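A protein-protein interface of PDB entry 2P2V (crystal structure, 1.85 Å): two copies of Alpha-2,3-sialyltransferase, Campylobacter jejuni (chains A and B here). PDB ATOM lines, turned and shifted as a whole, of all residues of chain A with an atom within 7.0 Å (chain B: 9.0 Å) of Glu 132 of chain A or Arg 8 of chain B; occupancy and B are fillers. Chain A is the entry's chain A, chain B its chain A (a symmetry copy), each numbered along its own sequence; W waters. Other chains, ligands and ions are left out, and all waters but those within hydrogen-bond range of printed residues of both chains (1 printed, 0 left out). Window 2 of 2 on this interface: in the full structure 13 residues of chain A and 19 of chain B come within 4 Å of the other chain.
Water W1 bridges OH of Tyr 77 of chain B (2.7 Å) and O of Ala 135 of chain A (2.8 Å).
The side-chain carboxylate (OD2) of Asp 119 of chain B is in salt-bridge range of the side-chain amino group (NZ) of Lys 81 of chain B (2.8 Å).
OH of Tyr 77 of chain B lies within hydrogen-bond range of OD1 of Asp 119 of chain B, 2.4 Å away.
Printed residues of chain B within 4 Å of Glu 132 of chain A: Arg 8 (3.99 Å).
Printed residues of chain A within 4 Å of Arg 8 of chain B: Glu 132 (3.99 Å).
Printed residues of chain B within 4 Å of Ala 135 of chain A: Pro 118 (3.9 Å) and Asp 119 (3.5 Å).
Of the printed residues of chain A, Asp 119 of chain B touches Ala 135 (3.5 Å).
Of the printed residues of chain B, Tyr 134 of chain A touches Pro 118.
No position is printed for both chains.
Among the printed residues, merely in contact across the chains: Lys 131 of chain A with Asn 11 of chain B (3.3 Å), Glu 132 of chain A with Arg 8 of chain B (3.99 Å), Tyr 134 of chain A with Pro 118 of chain B (3.96 Å), Ala 135 of chain A with Pro 118 of chain B (3.9 Å) and Ala 135 of chain A with Asp 119 of chain B (3.5 Å).
Of the 13 printed residues of chain A, 4 touch a printed residue of chain B.
Hydrophobic or aromatic side chains of chain A within 4 Å of the printed part of chain B: Tyr 134 and Ala 135.
Among the printed residues, no Asp or Glu carboxylate lies within 4 Å of a Lys or Arg side-chain nitrogen of the other chain.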
ATOM      1  N   GLU A 128      -6.505  -0.185  36.068  1.00  0.00           N
ATOM      2  CA  GLU A 128      -6.997  -1.426  35.492  1.00  0.00           C
ATOM      3  C   GLU A 128      -8.219  -1.923  36.310  1.00  0.00           C
ATOM      4  O   GLU A 128      -8.971  -2.777  35.858  1.00  0.00           O
ATOM      5  CB  GLU A 128      -5.931  -2.516  35.424  1.00  0.00           C
ATOM      6  CG  GLU A 128      -5.334  -2.943  36.761  1.00  0.00           C
ATOM      7  CD  GLU A 128      -4.200  -3.949  36.640  1.00  0.00           C
ATOM      8  OE1 GLU A 128      -3.753  -4.284  35.503  1.00  0.00           O
ATOM      9  OE2 GLU A 128      -3.699  -4.378  37.704  1.00  0.00           O
ATOM     10  N   ASN A 129      -8.322  -1.390  37.514  1.00  0.00           N
ATOM     11  CA  ASN A 129      -9.417  -1.773  38.409  1.00  0.00           C
ATOM     12  C   ASN A 129     -10.743  -1.144  38.029  1.00  0.00           C
ATOM     13  O   ASN A 129     -11.832  -1.591  38.538  1.00  0.00           O
ATOM     14  CB  ASN A 129      -9.060  -1.432  39.831  1.00  0.00           C
ATOM     15  CG  ASN A 129      -7.881  -2.254  40.334  1.00  0.00           C
ATOM     16  OD1 ASN A 129      -7.847  -3.477  40.177  1.00  0.00           O
ATOM     17  ND2 ASN A 129      -6.867  -1.567  40.868  1.00  0.00           N
ATOM     18  N   LEU A 130     -10.700  -0.115  37.191  1.00  0.00           N
ATOM     19  CA  LEU A 130     -11.898   0.488  36.611  1.00  0.00           C
ATOM     20  C   LEU A 130     -12.255  -0.324  35.361  1.00  0.00           C
ATOM     21  O   LEU A 130     -12.012   0.083  34.214  1.00  0.00           O
ATOM     22  CB  LEU A 130     -11.730   1.998  36.342  1.00  0.00           C
ATOM     23  CG  LEU A 130     -11.244   2.917  37.459  1.00  0.00           C
ATOM     24  CD1 LEU A 130     -11.061   4.305  36.928  1.00  0.00           C
ATOM     25  CD2 LEU A 130     -12.323   2.923  38.549  1.00  0.00           C
ATOM     26  N   LYS A 131     -12.832  -1.511  35.575  1.00  0.00           N
ATOM     27  CA  LYS A 131     -12.888  -2.496  34.505  1.00  0.00           C
ATOM     28  C   LYS A 131     -13.531  -2.004  33.255  1.00  0.00           C
ATOM     29  O   LYS A 131     -12.955  -2.147  32.151  1.00  0.00           O
ATOM     30  CB  LYS A 131     -13.491  -3.823  34.988  1.00  0.00           C
ATOM     31  CG  LYS A 131     -12.660  -4.437  36.121  1.00  0.00           C
ATOM     32  CD  LYS A 131     -13.096  -5.882  36.379  1.00  0.00           C
ATOM     33  CE  LYS A 131     -12.195  -6.570  37.408  1.00  0.00           C
ATOM     34  NZ  LYS A 131     -10.736  -6.342  37.139  1.00  0.00           N
ATOM     35  N   GLU A 132     -14.718  -1.394  33.392  1.00  0.00           N
ATOM     36  CA  GLU A 132     -15.430  -0.956  32.235  1.00  0.00           C
ATOM     37  C   GLU A 132     -14.677   0.186  31.509  1.00  0.00           C
ATOM     38  O   GLU A 132     -14.560   0.172  30.259  1.00  0.00           O
ATOM     39  CB  GLU A 132     -16.858  -0.546  32.632  1.00  0.00           C
ATOM     40  CG  GLU A 132     -17.600   0.101  31.487  1.00  0.00           C
ATOM     41  CD  GLU A 132     -19.101   0.296  31.729  1.00  0.00           C
ATOM     42  OE1 GLU A 132     -19.562  -0.010  32.858  1.00  0.00           O
ATOM     43  OE2 GLU A 132     -19.770   0.768  30.762  1.00  0.00           O
ATOM     44  N   PHE A 133     -14.142   1.134  32.277  1.00  0.00           N
ATOM     45  CA  PHE A 133     -13.486   2.338  31.705  1.00  0.00           C
ATOM     46  C   PHE A 133     -12.178   1.893  31.032  1.00  0.00           C
ATOM     47  O   PHE A 133     -11.856   2.299  29.877  1.00  0.00           O
ATOM     48  CB  PHE A 133     -13.184   3.366  32.790  1.00  0.00           C
ATOM     49  CG  PHE A 133     -12.521   4.594  32.253  1.00  0.00           C
ATOM     50  CD1 PHE A 133     -13.250   5.557  31.562  1.00  0.00           C
ATOM     51  CD2 PHE A 133     -11.112   4.760  32.396  1.00  0.00           C
ATOM     52  CE1 PHE A 133     -12.639   6.710  31.046  1.00  0.00           C
ATOM     53  CE2 PHE A 133     -10.462   5.934  31.835  1.00  0.00           C
ATOM     54  CZ  PHE A 133     -11.208   6.883  31.174  1.00  0.00           C
ATOM     55  N   TYR A 134     -11.496   0.984  31.694  1.00  0.00           N
ATOM     56  CA  TYR A 134     -10.194   0.462  31.177  1.00  0.00           C
ATOM     57  C   TYR A 134     -10.376  -0.267  29.858  1.00  0.00           C
ATOM     58  O   TYR A 134      -9.595  -0.084  28.918  1.00  0.00           O
ATOM     59  CB  TYR A 134      -9.601  -0.486  32.194  1.00  0.00           C
ATOM     60  CG  TYR A 134      -8.134  -0.865  31.974  1.00  0.00           C
ATOM     61  CD1 TYR A 134      -7.745  -2.189  31.872  1.00  0.00           C
ATOM     62  CD2 TYR A 134      -7.145   0.132  32.078  1.00  0.00           C
ATOM     63  CE1 TYR A 134      -6.364  -2.545  31.828  1.00  0.00           C
ATOM     64  CE2 TYR A 134      -5.754  -0.204  31.992  1.00  0.00           C
ATOM     65  CZ  TYR A 134      -5.394  -1.524  31.877  1.00  0.00           C
ATOM     66  OH  TYR A 134      -4.031  -1.847  31.809  1.00  0.00           O
ATOM     67  N   ALA A 135     -11.402  -1.129  29.757  1.00  0.00           N
ATOM     68  CA  ALA A 135     -11.695  -1.767  28.488  1.00  0.00           C
ATOM     69  C   ALA A 135     -12.092  -0.769  27.418  1.00  0.00           C
ATOM     70  O   ALA A 135     -11.745  -0.930  26.233  1.00  0.00           O
ATOM     71  CB  ALA A 135     -12.793  -2.856  28.662  1.00  0.00           C
ATOM     72  N   TYR A 136     -12.848   0.263  27.794  1.00  0.00           N
ATOM     73  CA  TYR A 136     -13.258   1.281  26.830  1.00  0.00           C
ATOM     74  C   TYR A 136     -12.063   2.097  26.294  1.00  0.00           C
ATOM     75  O   TYR A 136     -11.939   2.332  25.059  1.00  0.00           O
ATOM     76  CB  TYR A 136     -14.304   2.204  27.523  1.00  0.00           C
ATOM     77  CG  TYR A 136     -14.409   3.614  27.005  1.00  0.00           C
ATOM     78  CD1 TYR A 136     -13.690   4.628  27.593  1.00  0.00           C
ATOM     79  CD2 TYR A 136     -15.283   3.949  25.960  1.00  0.00           C
ATOM     80  CE1 TYR A 136     -13.774   5.917  27.151  1.00  0.00           C
ATOM     81  CE2 TYR A 136     -15.395   5.288  25.500  1.00  0.00           C
ATOM     82  CZ  TYR A 136     -14.631   6.255  26.127  1.00  0.00           C
ATOM     83  OH  TYR A 136     -14.669   7.576  25.735  1.00  0.00           O
ATOM     84  N   ILE A 137     -11.152   2.475  27.170  1.00  0.00           N
ATOM     85  CA  ILE A 137      -9.933   3.238  26.653  1.00  0.00           C
ATOM     86  C   ILE A 137      -9.034   2.354  25.840  1.00  0.00           C
ATOM     87  O   ILE A 137      -8.433   2.823  24.846  1.00  0.00           O
ATOM     88  CB  ILE A 137      -9.211   4.035  27.761  1.00  0.00           C
ATOM     89  CG1 ILE A 137      -8.523   3.125  28.839  1.00  0.00           C
ATOM     90  CG2 ILE A 137     -10.203   5.048  28.440  1.00  0.00           C
ATOM     91  CD1 ILE A 137      -7.631   3.893  29.869  1.00  0.00           C
ATOM     92  N   LEU A 216     -18.067   9.685  30.801  1.00  0.00           N
ATOM     93  CA  LEU A 216     -18.161   8.257  31.122  1.00  0.00           C
ATOM     94  C   LEU A 216     -17.697   7.899  32.514  1.00  0.00           C
ATOM     95  O   LEU A 216     -18.342   7.081  33.172  1.00  0.00           O
ATOM     96  CB  LEU A 216     -17.466   7.378  30.068  1.00  0.00           C
ATOM     97  CG  LEU A 216     -17.666   5.856  30.219  1.00  0.00           C
ATOM     98  CD1 LEU A 216     -19.186   5.478  30.073  1.00  0.00           C
ATOM     99  CD2 LEU A 216     -16.821   5.048  29.217  1.00  0.00           C
ATOM    100  N   ILE A 220     -20.327   6.053  35.033  1.00  0.00           N
ATOM    101  CA  ILE A 220     -20.096   4.717  35.589  1.00  0.00           C
ATOM    102  C   ILE A 220     -19.830   4.709  37.083  1.00  0.00           C
ATOM    103  O   ILE A 220     -20.319   3.834  37.821  1.00  0.00           O
ATOM    104  CB  ILE A 220     -18.877   3.976  34.877  1.00  0.00           C
ATOM    105  CG1 ILE A 220     -19.067   3.899  33.385  1.00  0.00           C
ATOM    106  CG2 ILE A 220     -18.731   2.551  35.386  1.00  0.00           C
ATOM    107  CD1 ILE A 220     -17.743   3.413  32.701  1.00  0.00           C
ATOM    108  N   TYR A 221     -18.971   5.620  37.539  1.00  0.00           N
ATOM    109  CA  TYR A 221     -18.432   5.510  38.901  1.00  0.00           C
ATOM    110  C   TYR A 221     -19.101   6.464  39.889  1.00  0.00           C
ATOM    111  O   TYR A 221     -18.783   6.455  41.071  1.00  0.00           O
ATOM    112  CB  TYR A 221     -16.874   5.627  38.915  1.00  0.00           C
ATOM    113  CG  TYR A 221     -16.298   4.528  38.023  1.00  0.00           C
ATOM    114  CD1 TYR A 221     -16.347   3.197  38.406  1.00  0.00           C
ATOM    115  CD2 TYR A 221     -15.823   4.819  36.766  1.00  0.00           C
ATOM    116  CE1 TYR A 221     -15.904   2.179  37.594  1.00  0.00           C
ATOM    117  CE2 TYR A 221     -15.368   3.809  35.931  1.00  0.00           C
ATOM    118  CZ  TYR A 221     -15.396   2.504  36.334  1.00  0.00           C
ATOM    119  OH  TYR A 221     -14.963   1.503  35.456  1.00  0.00           O
ATOM    120  N   ARG B   8     -19.855  -3.203  28.807  1.00  0.00           N
ATOM    121  CA  ARG B   8     -19.700  -3.996  30.078  1.00  0.00           C
ATOM    122  C   ARG B   8     -19.875  -5.520  29.885  1.00  0.00           C
ATOM    123  O   ARG B   8     -20.985  -6.009  29.632  1.00  0.00           O
ATOM    124  CB  ARG B   8     -20.658  -3.461  31.189  1.00  0.00           C
ATOM    125  N   MET B   9     -18.773  -6.262  29.993  1.00  0.00           N
ATOM    126  CA  MET B   9     -18.839  -7.717  30.087  1.00  0.00           C
ATOM    127  C   MET B   9     -19.087  -8.131  31.558  1.00  0.00           C
ATOM    128  O   MET B   9     -18.955  -7.308  32.471  1.00  0.00           O
ATOM    129  CB  MET B   9     -17.534  -8.352  29.595  1.00  0.00           C
ATOM    130  CG  MET B   9     -17.086  -8.022  28.176  1.00  0.00           C
ATOM    131  SD  MET B   9     -18.181  -8.665  26.902  1.00  0.00           S
ATOM    132  CE  MET B   9     -19.022  -7.167  26.473  1.00  0.00           C
ATOM    133  N   GLU B  10     -19.441  -9.398  31.782  1.00  0.00           N
ATOM    134  CA  GLU B  10     -19.395  -9.974  33.133  1.00  0.00           C
ATOM    135  C   GLU B  10     -17.934 -10.190  33.554  1.00  0.00           C
ATOM    136  O   GLU B  10     -17.109 -10.630  32.743  1.00  0.00           O
ATOM    137  CB  GLU B  10     -20.153 -11.323  33.197  1.00  0.00           C
ATOM    138  CG  GLU B  10     -21.691 -11.246  32.971  1.00  0.00           C
ATOM    139  CD  GLU B  10     -22.413 -12.626  32.891  1.00  0.00           C
ATOM    140  OE1 GLU B  10     -21.779 -13.696  32.771  1.00  0.00           O
ATOM    141  OE2 GLU B  10     -23.670 -12.617  32.916  1.00  0.00           O
ATOM    142  N   ASN B  11     -17.624  -9.911  34.820  1.00  0.00           N
ATOM    143  CA  ASN B  11     -16.298 -10.195  35.380  1.00  0.00           C
ATOM    144  C   ASN B  11     -15.986 -11.671  35.443  1.00  0.00           C
ATOM    145  O   ASN B  11     -14.835 -12.086  35.267  1.00  0.00           O
ATOM    146  CB  ASN B  11     -16.167  -9.609  36.783  1.00  0.00           C
ATOM    147  CG  ASN B  11     -15.943  -8.120  36.765  1.00  0.00           C
ATOM    148  OD1 ASN B  11     -15.923  -7.476  37.822  1.00  0.00           O
ATOM    149  ND2 ASN B  11     -15.779  -7.553  35.568  1.00  0.00           N
ATOM    150  N   ILE B  63     -26.757 -13.447  24.025  1.00  0.00           N
ATOM    151  CA  ILE B  63     -25.703 -14.450  24.069  1.00  0.00           C
ATOM    152  C   ILE B  63     -24.942 -14.412  25.410  1.00  0.00           C
ATOM    153  O   ILE B  63     -24.437 -13.345  25.842  1.00  0.00           O
ATOM    154  CB  ILE B  63     -24.728 -14.328  22.822  1.00  0.00           C
ATOM    155  CG1 ILE B  63     -25.500 -14.440  21.510  1.00  0.00           C
ATOM    156  CG2 ILE B  63     -23.730 -15.459  22.911  1.00  0.00           C
ATOM    157  CD1 ILE B  63     -24.732 -13.895  20.261  1.00  0.00           C
ATOM    158  N   TYR B  77     -13.082  -9.596  18.018  1.00  0.00           N
ATOM    159  CA  TYR B  77     -13.295  -8.763  19.239  1.00  0.00           C
ATOM    160  C   TYR B  77     -13.940  -7.423  18.870  1.00  0.00           C
ATOM    161  O   TYR B  77     -14.899  -6.998  19.448  1.00  0.00           O
ATOM    162  CB  TYR B  77     -11.951  -8.538  19.937  1.00  0.00           C
ATOM    163  CG  TYR B  77     -12.042  -7.766  21.236  1.00  0.00           C
ATOM    164  CD1 TYR B  77     -12.407  -8.416  22.427  1.00  0.00           C
ATOM    165  CD2 TYR B  77     -11.802  -6.401  21.282  1.00  0.00           C
ATOM    166  CE1 TYR B  77     -12.502  -7.695  23.629  1.00  0.00           C
ATOM    167  CE2 TYR B  77     -11.883  -5.666  22.502  1.00  0.00           C
ATOM    168  CZ  TYR B  77     -12.198  -6.342  23.649  1.00  0.00           C
ATOM    169  OH  TYR B  77     -12.247  -5.578  24.788  1.00  0.00           O
ATOM    170  N   LYS B  81     -17.747  -6.006  19.767  1.00  0.00           N
ATOM    171  CA  LYS B  81     -17.959  -4.694  20.358  1.00  0.00           C
ATOM    172  C   LYS B  81     -18.903  -3.860  19.487  1.00  0.00           C
ATOM    173  O   LYS B  81     -19.761  -3.193  20.026  1.00  0.00           O
ATOM    174  CB  LYS B  81     -16.662  -3.914  20.529  1.00  0.00           C
ATOM    175  CG  LYS B  81     -15.693  -4.448  21.519  1.00  0.00           C
ATOM    176  CD  LYS B  81     -16.248  -4.155  22.928  1.00  0.00           C
ATOM    177  CE  LYS B  81     -15.328  -4.746  23.908  1.00  0.00           C
ATOM    178  NZ  LYS B  81     -15.729  -4.374  25.302  1.00  0.00           N
ATOM    179  N   ILE B  84     -22.470  -5.153  19.837  1.00  0.00           N
ATOM    180  CA  ILE B  84     -22.997  -4.720  21.142  1.00  0.00           C
ATOM    181  C   ILE B  84     -23.415  -3.245  21.106  1.00  0.00           C
ATOM    182  O   ILE B  84     -24.548  -2.902  21.480  1.00  0.00           O
ATOM    183  CB  ILE B  84     -21.965  -4.916  22.270  1.00  0.00           C
ATOM    184  CG1 ILE B  84     -21.697  -6.413  22.474  1.00  0.00           C
ATOM    185  CG2 ILE B  84     -22.385  -4.147  23.541  1.00  0.00           C
ATOM    186  CD1 ILE B  84     -20.399  -6.762  23.133  1.00  0.00           C
ATOM    187  N   LEU B  85     -22.480  -2.383  20.695  1.00  0.00           N
ATOM    188  CA  LEU B  85     -22.764  -0.959  20.479  1.00  0.00           C
ATOM    189  C   LEU B  85     -23.948  -0.665  19.540  1.00  0.00           C
ATOM    190  O   LEU B  85     -24.634   0.339  19.741  1.00  0.00           O
ATOM    191  CB  LEU B  85     -21.510  -0.231  19.941  1.00  0.00           C
ATOM    192  CG  LEU B  85     -20.298  -0.091  20.867  1.00  0.00           C
ATOM    193  CD1 LEU B  85     -19.084   0.367  20.072  1.00  0.00           C
ATOM    194  CD2 LEU B  85     -20.553   0.869  22.040  1.00  0.00           C
ATOM    195  N   GLU B  90     -26.727  -8.766  22.640  1.00  0.00           N
ATOM    196  CA  GLU B  90     -26.228  -8.554  23.964  1.00  0.00           C
ATOM    197  C   GLU B  90     -25.286  -9.736  24.192  1.00  0.00           C
ATOM    198  O   GLU B  90     -25.682 -10.912  24.040  1.00  0.00           O
ATOM    199  CB  GLU B  90     -27.397  -8.645  24.931  1.00  0.00           C
ATOM    200  CG  GLU B  90     -27.053  -8.351  26.352  1.00  0.00           C
ATOM    201  CD  GLU B  90     -28.260  -8.574  27.214  1.00  0.00           C
ATOM    202  OE1 GLU B  90     -29.245  -7.803  27.033  1.00  0.00           O
ATOM    203  OE2 GLU B  90     -28.231  -9.553  28.012  1.00  0.00           O
ATOM    204  N   ILE B  91     -24.042  -9.426  24.537  1.00  0.00           N
ATOM    205  CA  ILE B  91     -22.992 -10.455  24.682  1.00  0.00           C
ATOM    206  C   ILE B  91     -22.391 -10.249  26.041  1.00  0.00           C
ATOM    207  O   ILE B  91     -21.795  -9.164  26.318  1.00  0.00           O
ATOM    208  CB  ILE B  91     -21.936 -10.301  23.593  1.00  0.00           C
ATOM    209  CG1 ILE B  91     -22.580 -10.541  22.228  1.00  0.00           C
ATOM    210  CG2 ILE B  91     -20.755 -11.302  23.849  1.00  0.00           C
ATOM    211  CD1 ILE B  91     -21.703 -10.201  21.005  1.00  0.00           C
ATOM    212  N   LYS B  92     -22.567 -11.238  26.929  1.00  0.00           N
ATOM    213  CA  LYS B  92     -22.082 -11.105  28.281  1.00  0.00           C
ATOM    214  C   LYS B  92     -20.622 -11.446  28.520  1.00  0.00           C
ATOM    215  O   LYS B  92     -20.037 -10.960  29.485  1.00  0.00           O
ATOM    216  CB  LYS B  92     -22.978 -11.833  29.292  1.00  0.00           C
ATOM    217  CG  LYS B  92     -24.369 -11.177  29.369  1.00  0.00           C
ATOM    218  CD  LYS B  92     -25.362 -12.141  30.027  1.00  0.00           C
ATOM    219  CE  LYS B  92     -26.603 -11.398  30.493  1.00  0.00           C
ATOM    220  NZ  LYS B  92     -26.212 -10.425  31.551  1.00  0.00           N
ATOM    221  N   ASN B  93     -20.034 -12.255  27.647  1.00  0.00           N
ATOM    222  CA  ASN B  93     -18.666 -12.700  27.874  1.00  0.00           C
ATOM    223  C   ASN B  93     -18.050 -12.966  26.527  1.00  0.00           C
ATOM    224  O   ASN B  93     -18.706 -13.438  25.644  1.00  0.00           O
ATOM    225  CB  ASN B  93     -18.617 -14.068  28.586  1.00  0.00           C
ATOM    226  CG  ASN B  93     -19.070 -13.995  30.044  1.00  0.00           C
ATOM    227  OD1 ASN B  93     -18.256 -13.768  30.905  1.00  0.00           O
ATOM    228  ND2 ASN B  93     -20.369 -14.235  30.313  1.00  0.00           N
ATOM    229  N   ILE B  94     -16.746 -12.790  26.426  1.00  0.00           N
ATOM    230  CA  ILE B  94     -16.084 -13.066  25.138  1.00  0.00           C
ATOM    231  C   ILE B  94     -14.872 -13.939  25.392  1.00  0.00           C
ATOM    232  O   ILE B  94     -13.971 -13.518  26.114  1.00  0.00           O
ATOM    233  CB  ILE B  94     -15.578 -11.757  24.427  1.00  0.00           C
ATOM    234  CG1 ILE B  94     -16.743 -10.837  24.093  1.00  0.00           C
ATOM    235  CG2 ILE B  94     -14.835 -12.183  23.145  1.00  0.00           C
ATOM    236  CD1 ILE B  94     -16.315  -9.410  23.556  1.00  0.00           C
ATOM    237  N   PRO B 118      -8.658  -6.649  27.646  1.00  0.00           N
ATOM    238  CA  PRO B 118      -8.689  -6.779  29.106  1.00  0.00           C
ATOM    239  C   PRO B 118      -9.941  -7.418  29.666  1.00  0.00           C
ATOM    240  O   PRO B 118      -9.893  -7.990  30.752  1.00  0.00           O
ATOM    241  CB  PRO B 118      -8.493  -5.338  29.590  1.00  0.00           C
ATOM    242  CG  PRO B 118      -8.900  -4.477  28.446  1.00  0.00           C
ATOM    243  CD  PRO B 118      -8.532  -5.232  27.239  1.00  0.00           C
ATOM    244  N   ASP B 119     -11.035  -7.314  28.932  1.00  0.00           N
ATOM    245  CA  ASP B 119     -12.330  -7.890  29.335  1.00  0.00           C
ATOM    246  C   ASP B 119     -12.685  -9.177  28.629  1.00  0.00           C
ATOM    247  O   ASP B 119     -13.800  -9.704  28.824  1.00  0.00           O
ATOM    248  CB  ASP B 119     -13.438  -6.852  29.185  1.00  0.00           C
ATOM    249  CG  ASP B 119     -13.658  -6.379  27.771  1.00  0.00           C
ATOM    250  OD1 ASP B 119     -12.849  -6.716  26.859  1.00  0.00           O
ATOM    251  OD2 ASP B 119     -14.639  -5.651  27.590  1.00  0.00           O
HETATM  252  O   HOH W   1     -10.710  -3.354  25.249  1.00  0.00           O
